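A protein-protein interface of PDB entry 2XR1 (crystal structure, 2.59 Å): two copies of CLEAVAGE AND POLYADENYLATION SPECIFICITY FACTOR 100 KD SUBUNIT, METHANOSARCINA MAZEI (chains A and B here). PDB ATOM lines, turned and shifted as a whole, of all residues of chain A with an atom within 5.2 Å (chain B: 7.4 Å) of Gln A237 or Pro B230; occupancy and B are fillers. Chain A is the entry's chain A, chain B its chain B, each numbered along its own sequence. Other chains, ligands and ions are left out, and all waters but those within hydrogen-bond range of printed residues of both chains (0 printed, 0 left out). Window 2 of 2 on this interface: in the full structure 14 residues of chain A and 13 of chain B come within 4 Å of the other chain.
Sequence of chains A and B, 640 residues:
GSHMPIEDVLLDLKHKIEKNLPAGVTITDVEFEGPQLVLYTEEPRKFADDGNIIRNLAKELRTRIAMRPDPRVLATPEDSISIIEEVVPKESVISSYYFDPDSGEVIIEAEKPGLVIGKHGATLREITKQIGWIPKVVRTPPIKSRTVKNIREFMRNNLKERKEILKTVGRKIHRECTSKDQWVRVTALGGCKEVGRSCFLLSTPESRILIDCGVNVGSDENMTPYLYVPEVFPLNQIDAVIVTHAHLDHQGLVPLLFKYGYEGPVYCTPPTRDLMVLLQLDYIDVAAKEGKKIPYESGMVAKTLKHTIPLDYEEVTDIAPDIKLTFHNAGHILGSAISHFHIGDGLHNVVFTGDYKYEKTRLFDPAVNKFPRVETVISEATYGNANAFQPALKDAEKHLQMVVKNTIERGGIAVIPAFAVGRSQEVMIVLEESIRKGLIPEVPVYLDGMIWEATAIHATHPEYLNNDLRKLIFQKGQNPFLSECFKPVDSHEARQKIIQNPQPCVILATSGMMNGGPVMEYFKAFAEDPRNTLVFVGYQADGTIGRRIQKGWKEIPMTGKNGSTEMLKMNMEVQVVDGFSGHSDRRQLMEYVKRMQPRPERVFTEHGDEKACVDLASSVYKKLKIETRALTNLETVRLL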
ATOM      1  N   ARG A 185     -15.130  20.987 -13.744  1.00  0.00           N
ATOM      2  CA  ARG A 185     -15.613  20.429 -12.508  1.00  0.00           C
ATOM      3  C   ARG A 185     -16.721  19.382 -12.709  1.00  0.00           C
ATOM      4  O   ARG A 185     -17.277  19.287 -13.786  1.00  0.00           O
ATOM      5  CB  ARG A 185     -16.094  21.546 -11.644  1.00  0.00           C
ATOM      6  CG  ARG A 185     -17.014  22.464 -12.334  1.00  0.00           C
ATOM      7  CD  ARG A 185     -17.275  23.689 -11.484  1.00  0.00           C
ATOM      8  NE  ARG A 185     -18.507  24.323 -11.953  1.00  0.00           N
ATOM      9  CZ  ARG A 185     -19.423  24.905 -11.202  1.00  0.00           C
ATOM     10  NH1 ARG A 185     -19.283  25.022  -9.885  1.00  0.00           N
ATOM     11  NH2 ARG A 185     -20.460  25.433 -11.777  1.00  0.00           N
ATOM     12  N   ARG A 208     -21.825  21.723 -20.567  1.00  0.00           N
ATOM     13  CA  ARG A 208     -22.396  20.931 -19.494  1.00  0.00           C
ATOM     14  C   ARG A 208     -22.793  19.612 -20.117  1.00  0.00           C
ATOM     15  O   ARG A 208     -23.526  19.597 -21.084  1.00  0.00           O
ATOM     16  CB  ARG A 208     -23.593  21.658 -18.865  1.00  0.00           C
ATOM     17  CG  ARG A 208     -23.139  22.837 -17.995  1.00  0.00           C
ATOM     18  CD  ARG A 208     -24.017  24.052 -18.124  1.00  0.00           C
ATOM     19  NE  ARG A 208     -24.103  24.499 -19.521  1.00  0.00           N
ATOM     20  CZ  ARG A 208     -23.326  25.419 -20.105  1.00  0.00           C
ATOM     21  NH1 ARG A 208     -22.362  26.029 -19.443  1.00  0.00           N
ATOM     22  NH2 ARG A 208     -23.513  25.720 -21.390  1.00  0.00           N
ATOM     23  N   PRO A 230     -30.255  24.184  -9.566  1.00  0.00           N
ATOM     24  CA  PRO A 230     -29.731  25.151 -10.527  1.00  0.00           C
ATOM     25  C   PRO A 230     -28.696  24.612 -11.549  1.00  0.00           C
ATOM     26  O   PRO A 230     -28.630  25.128 -12.656  1.00  0.00           O
ATOM     27  CB  PRO A 230     -29.115  26.193  -9.626  1.00  0.00           C
ATOM     28  CG  PRO A 230     -29.967  26.158  -8.408  1.00  0.00           C
ATOM     29  CD  PRO A 230     -30.252  24.730  -8.198  1.00  0.00           C
ATOM     30  N   GLU A 231     -27.922  23.584 -11.209  1.00  0.00           N
ATOM     31  CA  GLU A 231     -26.883  23.066 -12.095  1.00  0.00           C
ATOM     32  C   GLU A 231     -27.466  22.224 -13.229  1.00  0.00           C
ATOM     33  O   GLU A 231     -26.773  21.856 -14.172  1.00  0.00           O
ATOM     34  CB  GLU A 231     -25.920  22.140 -11.341  1.00  0.00           C
ATOM     35  CG  GLU A 231     -25.199  22.730 -10.182  1.00  0.00           C
ATOM     36  CD  GLU A 231     -25.994  22.674  -8.897  1.00  0.00           C
ATOM     37  OE1 GLU A 231     -27.152  23.198  -8.785  1.00  0.00           O
ATOM     38  OE2 GLU A 231     -25.438  22.103  -7.964  1.00  0.00           O
ATOM     39  N   VAL A 232     -28.719  21.844 -13.121  1.00  0.00           N
ATOM     40  CA  VAL A 232     -29.344  21.061 -14.169  1.00  0.00           C
ATOM     41  C   VAL A 232     -30.557  21.765 -14.817  1.00  0.00           C
ATOM     42  O   VAL A 232     -30.814  21.593 -16.003  1.00  0.00           O
ATOM     43  CB  VAL A 232     -29.720  19.708 -13.612  1.00  0.00           C
ATOM     44  CG1 VAL A 232     -30.976  19.167 -14.246  1.00  0.00           C
ATOM     45  CG2 VAL A 232     -28.579  18.764 -13.829  1.00  0.00           C
ATOM     46  N   PHE A 233     -31.284  22.563 -14.054  1.00  0.00           N
ATOM     47  CA  PHE A 233     -32.336  23.430 -14.615  1.00  0.00           C
ATOM     48  C   PHE A 233     -31.800  24.840 -14.913  1.00  0.00           C
ATOM     49  O   PHE A 233     -31.302  25.496 -13.997  1.00  0.00           O
ATOM     50  CB  PHE A 233     -33.494  23.580 -13.636  1.00  0.00           C
ATOM     51  CG  PHE A 233     -34.509  22.504 -13.748  1.00  0.00           C
ATOM     52  CD1 PHE A 233     -34.155  21.179 -13.588  1.00  0.00           C
ATOM     53  CD2 PHE A 233     -35.836  22.820 -14.012  1.00  0.00           C
ATOM     54  CE1 PHE A 233     -35.115  20.156 -13.703  1.00  0.00           C
ATOM     55  CE2 PHE A 233     -36.811  21.811 -14.141  1.00  0.00           C
ATOM     56  CZ  PHE A 233     -36.445  20.471 -13.982  1.00  0.00           C
ATOM     57  N   PRO A 234     -31.989  25.344 -16.161  1.00  0.00           N
ATOM     58  CA  PRO A 234     -32.892  24.770 -17.170  1.00  0.00           C
ATOM     59  C   PRO A 234     -32.203  23.732 -18.017  1.00  0.00           C
ATOM     60  O   PRO A 234     -31.061  23.910 -18.401  1.00  0.00           O
ATOM     61  CB  PRO A 234     -33.269  25.985 -18.023  1.00  0.00           C
ATOM     62  CG  PRO A 234     -32.019  26.844 -18.013  1.00  0.00           C
ATOM     63  CD  PRO A 234     -31.227  26.479 -16.731  1.00  0.00           C
ATOM     64  N   LEU A 235     -32.908  22.644 -18.284  1.00  0.00           N
ATOM     65  CA  LEU A 235     -32.370  21.525 -19.040  1.00  0.00           C
ATOM     66  C   LEU A 235     -31.840  21.837 -20.440  1.00  0.00           C
ATOM     67  O   LEU A 235     -31.054  21.050 -20.969  1.00  0.00           O
ATOM     68  CB  LEU A 235     -33.416  20.426 -19.146  1.00  0.00           C
ATOM     69  CG  LEU A 235     -33.738  19.737 -17.831  1.00  0.00           C
ATOM     70  CD1 LEU A 235     -35.021  18.997 -17.972  1.00  0.00           C
ATOM     71  CD2 LEU A 235     -32.653  18.782 -17.467  1.00  0.00           C
ATOM     72  N   ASN A 236     -32.253  22.945 -21.043  1.00  0.00           N
ATOM     73  CA  ASN A 236     -31.639  23.393 -22.302  1.00  0.00           C
ATOM     74  C   ASN A 236     -30.137  23.764 -22.165  1.00  0.00           C
ATOM     75  O   ASN A 236     -29.370  23.752 -23.125  1.00  0.00           O
ATOM     76  CB  ASN A 236     -32.453  24.538 -22.947  1.00  0.00           C
ATOM     77  CG  ASN A 236     -32.292  25.914 -22.222  1.00  0.00           C
ATOM     78  OD1 ASN A 236     -31.400  26.116 -21.373  1.00  0.00           O
ATOM     79  ND2 ASN A 236     -33.164  26.864 -22.585  1.00  0.00           N
ATOM     80  N   GLN A 237     -29.691  24.046 -20.957  1.00  0.00           N
ATOM     81  CA  GLN A 237     -28.282  24.321 -20.759  1.00  0.00           C
ATOM     82  C   GLN A 237     -27.398  23.068 -20.928  1.00  0.00           C
ATOM     83  O   GLN A 237     -26.155  23.169 -20.904  1.00  0.00           O
ATOM     84  CB  GLN A 237     -28.071  24.943 -19.366  1.00  0.00           C
ATOM     85  CG  GLN A 237     -27.848  23.913 -18.250  1.00  0.00           C
ATOM     86  CD  GLN A 237     -27.689  24.537 -16.883  1.00  0.00           C
ATOM     87  OE1 GLN A 237     -26.577  24.636 -16.396  1.00  0.00           O
ATOM     88  NE2 GLN A 237     -28.814  24.929 -16.242  1.00  0.00           N
ATOM     89  N   ILE A 238     -28.023  21.897 -21.075  1.00  0.00           N
ATOM     90  CA  ILE A 238     -27.266  20.674 -21.169  1.00  0.00           C
ATOM     91  C   ILE A 238     -26.904  20.345 -22.621  1.00  0.00           C
ATOM     92  O   ILE A 238     -27.778  20.075 -23.441  1.00  0.00           O
ATOM     93  CB  ILE A 238     -27.994  19.470 -20.557  1.00  0.00           C
ATOM     94  CG1 ILE A 238     -28.495  19.778 -19.166  1.00  0.00           C
ATOM     95  CG2 ILE A 238     -27.042  18.340 -20.461  1.00  0.00           C
ATOM     96  CD1 ILE A 238     -27.391  19.913 -18.175  1.00  0.00           C
ATOM     97  N   ASP A 239     -25.609  20.341 -22.917  1.00  0.00           N
ATOM     98  CA  ASP A 239     -25.136  20.017 -24.249  1.00  0.00           C
ATOM     99  C   ASP A 239     -25.413  18.572 -24.644  1.00  0.00           C
ATOM    100  O   ASP A 239     -25.797  18.333 -25.796  1.00  0.00           O
ATOM    101  CB  ASP A 239     -23.640  20.311 -24.371  1.00  0.00           C
ATOM    102  CG  ASP A 239     -23.334  21.807 -24.321  1.00  0.00           C
ATOM    103  OD1 ASP A 239     -23.778  22.510 -23.367  1.00  0.00           O
ATOM    104  OD2 ASP A 239     -22.652  22.288 -25.255  1.00  0.00           O
ATOM    105  N   LEU B 201     -22.332  30.979  -1.989  1.00  0.00           N
ATOM    106  CA  LEU B 201     -23.768  30.719  -2.148  1.00  0.00           C
ATOM    107  C   LEU B 201     -24.163  29.690  -1.129  1.00  0.00           C
ATOM    108  O   LEU B 201     -23.571  28.660  -1.114  1.00  0.00           O
ATOM    109  CB  LEU B 201     -24.077  30.224  -3.535  1.00  0.00           C
ATOM    110  CG  LEU B 201     -25.565  30.168  -3.833  1.00  0.00           C
ATOM    111  CD1 LEU B 201     -26.073  31.564  -4.047  1.00  0.00           C
ATOM    112  CD2 LEU B 201     -25.856  29.160  -5.062  1.00  0.00           C
ATOM    113  N   ARG B 208     -31.732  30.393  -1.978  1.00  0.00           N
ATOM    114  CA  ARG B 208     -30.388  30.670  -2.413  1.00  0.00           C
ATOM    115  C   ARG B 208     -30.010  32.010  -1.852  1.00  0.00           C
ATOM    116  O   ARG B 208     -30.733  32.983  -2.036  1.00  0.00           O
ATOM    117  CB  ARG B 208     -30.344  30.640  -3.933  1.00  0.00           C
ATOM    118  CG  ARG B 208     -30.424  29.206  -4.482  1.00  0.00           C
ATOM    119  CD  ARG B 208     -31.162  29.127  -5.750  1.00  0.00           C
ATOM    120  NE  ARG B 208     -32.546  29.588  -5.589  1.00  0.00           N
ATOM    121  CZ  ARG B 208     -33.605  28.822  -5.270  1.00  0.00           C
ATOM    122  NH1 ARG B 208     -33.477  27.510  -5.066  1.00  0.00           N
ATOM    123  NH2 ARG B 208     -34.816  29.386  -5.138  1.00  0.00           N
ATOM    124  N   TYR B 226     -16.857  34.264  -9.817  1.00  0.00           N
ATOM    125  CA  TYR B 226     -17.484  33.552 -10.923  1.00  0.00           C
ATOM    126  C   TYR B 226     -19.012  33.708 -10.858  1.00  0.00           C
ATOM    127  O   TYR B 226     -19.732  32.788 -10.483  1.00  0.00           O
ATOM    128  CB  TYR B 226     -17.083  32.053 -10.931  1.00  0.00           C
ATOM    129  CG  TYR B 226     -15.613  31.808 -11.133  1.00  0.00           C
ATOM    130  CD1 TYR B 226     -15.084  31.738 -12.376  1.00  0.00           C
ATOM    131  CD2 TYR B 226     -14.763  31.702 -10.055  1.00  0.00           C
ATOM    132  CE1 TYR B 226     -13.707  31.557 -12.556  1.00  0.00           C
ATOM    133  CE2 TYR B 226     -13.427  31.530 -10.213  1.00  0.00           C
ATOM    134  CZ  TYR B 226     -12.904  31.461 -11.444  1.00  0.00           C
ATOM    135  OH  TYR B 226     -11.578  31.264 -11.594  1.00  0.00           O
ATOM    136  N   LEU B 227     -19.497  34.882 -11.241  1.00  0.00           N
ATOM    137  CA  LEU B 227     -20.917  35.177 -11.166  1.00  0.00           C
ATOM    138  C   LEU B 227     -21.709  34.610 -12.351  1.00  0.00           C
ATOM    139  O   LEU B 227     -22.935  34.671 -12.305  1.00  0.00           O
ATOM    140  CB  LEU B 227     -21.158  36.682 -11.087  1.00  0.00           C
ATOM    141  CG  LEU B 227     -20.631  37.410  -9.856  1.00  0.00           C
ATOM    142  CD1 LEU B 227     -20.869  38.938  -9.939  1.00  0.00           C
ATOM    143  CD2 LEU B 227     -21.233  36.813  -8.558  1.00  0.00           C
ATOM    144  N   TYR B 228     -21.061  34.041 -13.372  1.00  0.00           N
ATOM    145  CA  TYR B 228     -21.759  33.752 -14.637  1.00  0.00           C
ATOM    146  C   TYR B 228     -22.170  32.262 -14.750  1.00  0.00           C
ATOM    147  O   TYR B 228     -22.562  31.799 -15.817  1.00  0.00           O
ATOM    148  CB  TYR B 228     -20.928  34.270 -15.834  1.00  0.00           C
ATOM    149  CG  TYR B 228     -20.539  35.737 -15.634  1.00  0.00           C
ATOM    150  CD1 TYR B 228     -19.429  36.078 -14.861  1.00  0.00           C
ATOM    151  CD2 TYR B 228     -21.318  36.779 -16.151  1.00  0.00           C
ATOM    152  CE1 TYR B 228     -19.083  37.405 -14.639  1.00  0.00           C
ATOM    153  CE2 TYR B 228     -20.976  38.114 -15.929  1.00  0.00           C
ATOM    154  CZ  TYR B 228     -19.860  38.415 -15.172  1.00  0.00           C
ATOM    155  OH  TYR B 228     -19.497  39.719 -14.936  1.00  0.00           O
ATOM    156  N   VAL B 229     -22.121  31.537 -13.642  1.00  0.00           N
ATOM    157  CA  VAL B 229     -22.302  30.092 -13.613  1.00  0.00           C
ATOM    158  C   VAL B 229     -23.697  29.702 -13.247  1.00  0.00           C
ATOM    159  O   VAL B 229     -24.372  30.450 -12.586  1.00  0.00           O
ATOM    160  CB  VAL B 229     -21.377  29.419 -12.537  1.00  0.00           C
ATOM    161  CG1 VAL B 229     -19.942  29.543 -12.932  1.00  0.00           C
ATOM    162  CG2 VAL B 229     -21.631  29.965 -11.105  1.00  0.00           C
ATOM    163  N   PRO B 230     -24.122  28.486 -13.609  1.00  0.00           N
ATOM    164  CA  PRO B 230     -25.522  28.093 -13.435  1.00  0.00           C
ATOM    165  C   PRO B 230     -26.080  28.242 -12.035  1.00  0.00           C
ATOM    166  O   PRO B 230     -27.266  28.390 -11.895  1.00  0.00           O
ATOM    167  CB  PRO B 230     -25.504  26.626 -13.825  1.00  0.00           C
ATOM    168  CG  PRO B 230     -24.509  26.570 -14.837  1.00  0.00           C
ATOM    169  CD  PRO B 230     -23.411  27.481 -14.397  1.00  0.00           C
ATOM    170  N   GLU B 231     -25.234  28.229 -11.029  1.00  0.00           N
ATOM    171  CA  GLU B 231     -25.658  28.352  -9.634  1.00  0.00           C
ATOM    172  C   GLU B 231     -26.069  29.733  -9.249  1.00  0.00           C
ATOM    173  O   GLU B 231     -26.658  29.900  -8.209  1.00  0.00           O
ATOM    174  CB  GLU B 231     -24.501  27.991  -8.678  1.00  0.00           C
ATOM    175  CG  GLU B 231     -23.987  26.584  -8.786  1.00  0.00           C
ATOM    176  CD  GLU B 231     -22.990  26.374  -9.912  1.00  0.00           C
ATOM    177  OE1 GLU B 231     -23.250  26.720 -11.084  1.00  0.00           O
ATOM    178  OE2 GLU B 231     -21.937  25.824  -9.645  1.00  0.00           O
ATOM    179  N   VAL B 232     -25.677  30.731 -10.029  1.00  0.00           N
ATOM    180  CA  VAL B 232     -25.987  32.117  -9.720  1.00  0.00           C
ATOM    181  C   VAL B 232     -26.915  32.745 -10.757  1.00  0.00           C
ATOM    182  O   VAL B 232     -27.737  33.572 -10.393  1.00  0.00           O
ATOM    183  CB  VAL B 232     -24.703  32.905  -9.538  1.00  0.00           C
ATOM    184  CG1 VAL B 232     -24.887  34.391  -9.913  1.00  0.00           C
ATOM    185  CG2 VAL B 232     -24.282  32.779  -8.128  1.00  0.00           C
ATOM    186  N   PHE B 233     -26.760  32.370 -12.031  1.00  0.00           N
ATOM    187  CA  PHE B 233     -27.649  32.830 -13.100  1.00  0.00           C
ATOM    188  C   PHE B 233     -28.797  31.827 -13.217  1.00  0.00           C
ATOM    189  O   PHE B 233     -28.533  30.640 -13.338  1.00  0.00           O
ATOM    190  CB  PHE B 233     -26.902  32.959 -14.452  1.00  0.00           C
ATOM    191  CG  PHE B 233     -26.262  34.327 -14.683  1.00  0.00           C
ATOM    192  CD1 PHE B 233     -25.288  34.798 -13.827  1.00  0.00           C
ATOM    193  CD2 PHE B 233     -26.635  35.126 -15.782  1.00  0.00           C
ATOM    194  CE1 PHE B 233     -24.699  36.081 -14.038  1.00  0.00           C
ATOM    195  CE2 PHE B 233     -26.052  36.398 -16.003  1.00  0.00           C
ATOM    196  CZ  PHE B 233     -25.082  36.872 -15.132  1.00  0.00           C
ATOM    197  N   PRO B 234     -30.071  32.307 -13.228  1.00  0.00           N
ATOM    198  CA  PRO B 234     -30.446  33.719 -13.320  1.00  0.00           C
ATOM    199  C   PRO B 234     -30.503  34.323 -11.932  1.00  0.00           C
ATOM    200  O   PRO B 234     -31.004  33.699 -11.019  1.00  0.00           O
ATOM    201  CB  PRO B 234     -31.834  33.668 -13.945  1.00  0.00           C
ATOM    202  CG  PRO B 234     -32.428  32.408 -13.410  1.00  0.00           C
ATOM    203  CD  PRO B 234     -31.271  31.464 -13.053  1.00  0.00           C
ATOM    204  N   GLN B 237     -33.190  34.110  -9.157  1.00  0.00           N
ATOM    205  CA  GLN B 237     -33.245  32.943  -8.260  1.00  0.00           C
ATOM    206  C   GLN B 237     -32.599  33.226  -6.888  1.00  0.00           C
ATOM    207  O   GLN B 237     -32.590  32.336  -6.034  1.00  0.00           O
ATOM    208  CB  GLN B 237     -32.551  31.720  -8.910  1.00  0.00           C
ATOM    209  CG  GLN B 237     -31.031  31.589  -8.635  1.00  0.00           C
ATOM    210  CD  GLN B 237     -30.381  30.380  -9.327  1.00  0.00           C
ATOM    211  OE1 GLN B 237     -30.179  29.352  -8.694  1.00  0.00           O
ATOM    212  NE2 GLN B 237     -30.039  30.516 -10.637  1.00  0.00           N
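Of the printed residues of chain B, Arg A185 touches Glu B231 (2.6 Å). Of the printed residues of chain B, Pro A230 touches Pro B230 (3.6 Å) and Gln B237 (3.2 Å). Of chain B, only Pro B230 (3.2 Å) comes within 4 Å of Gln A237. Tyr B228 touches none of the printed residues of chain A. Of chain A, only Pro A230 and Gln A237 come within 4 Å of Pro B230. The nearest printed residue of chain A that does not touch Pro B230 is Arg A208 (4.2 Å). The nearest printed residue of chain A that does not touch Gln B237 is Phe A233 (6.2 Å).
NH2 of Arg A185 is in salt-bridge range of OE2 of Glu B231 (2.6 Å).
The guanidinium group (NE) of Arg A208 is in hydrogen-bond range of the backbone carbonyl oxygen (O) of Gln A237 (2.8 Å). O of Phe A233 sits close to NE2 of Gln A237 (3.4 Å). The backbone carbonyl oxygen (O) of Pro A234 sits close to the side-chain amide nitrogen (NE2) of Gln A237, at 3.3 Å. The backbone carbonyl oxygen of Gln B237 is in hydrogen-bond range of the guanidinium group of Arg B208, 2.8 Å away. The side-chain amide nitrogen (NE2) of Gln B237 is in hydrogen-bond range of the backbone carbonyl oxygen (O) of Phe B233. The side-chain amide nitrogen (NE2) of Gln B237 sits close to the backbone carbonyl oxygen (O) of Pro B234, at 3.3 Å.
Among the printed residues, pairs that only touch across the chains: Pro A230 with Pro B230, Pro A230 with Gln B237 and Gln A237 with Pro B230.
Pro A230 touches its own counterpart, Pro B230. Pro A230 touches Gln B237, and with the chains exchanged Gln A237 touches Pro B230. Positions printed for both chains: 208, 230, 231, 232, 233, 234 and 237. Of the 4 pairs that touch across the chains among the printed residues, 3 have their exchanged pair printed and touching as well.
Of the 12 printed residues of chain A, 3 touch a printed residue of chain B. Printed residues of chain A that touch a printed residue of chain B: Arg A185, Pro A230 and Gln A237. Of the 12 printed residues of chain B, 3 touch a printed residue of chain A. Hydrophobic or aromatic side chains of chain B within 4 Å of the printed part of chain A: Pro B230. Among the printed residues, 4 pairs touch across the chains. Among the printed residues, Asp or Glu carboxylates within 4 Å of a Lys or Arg side-chain nitrogen of the other chain: Arg A185 with Glu B231 (2.6 Å).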
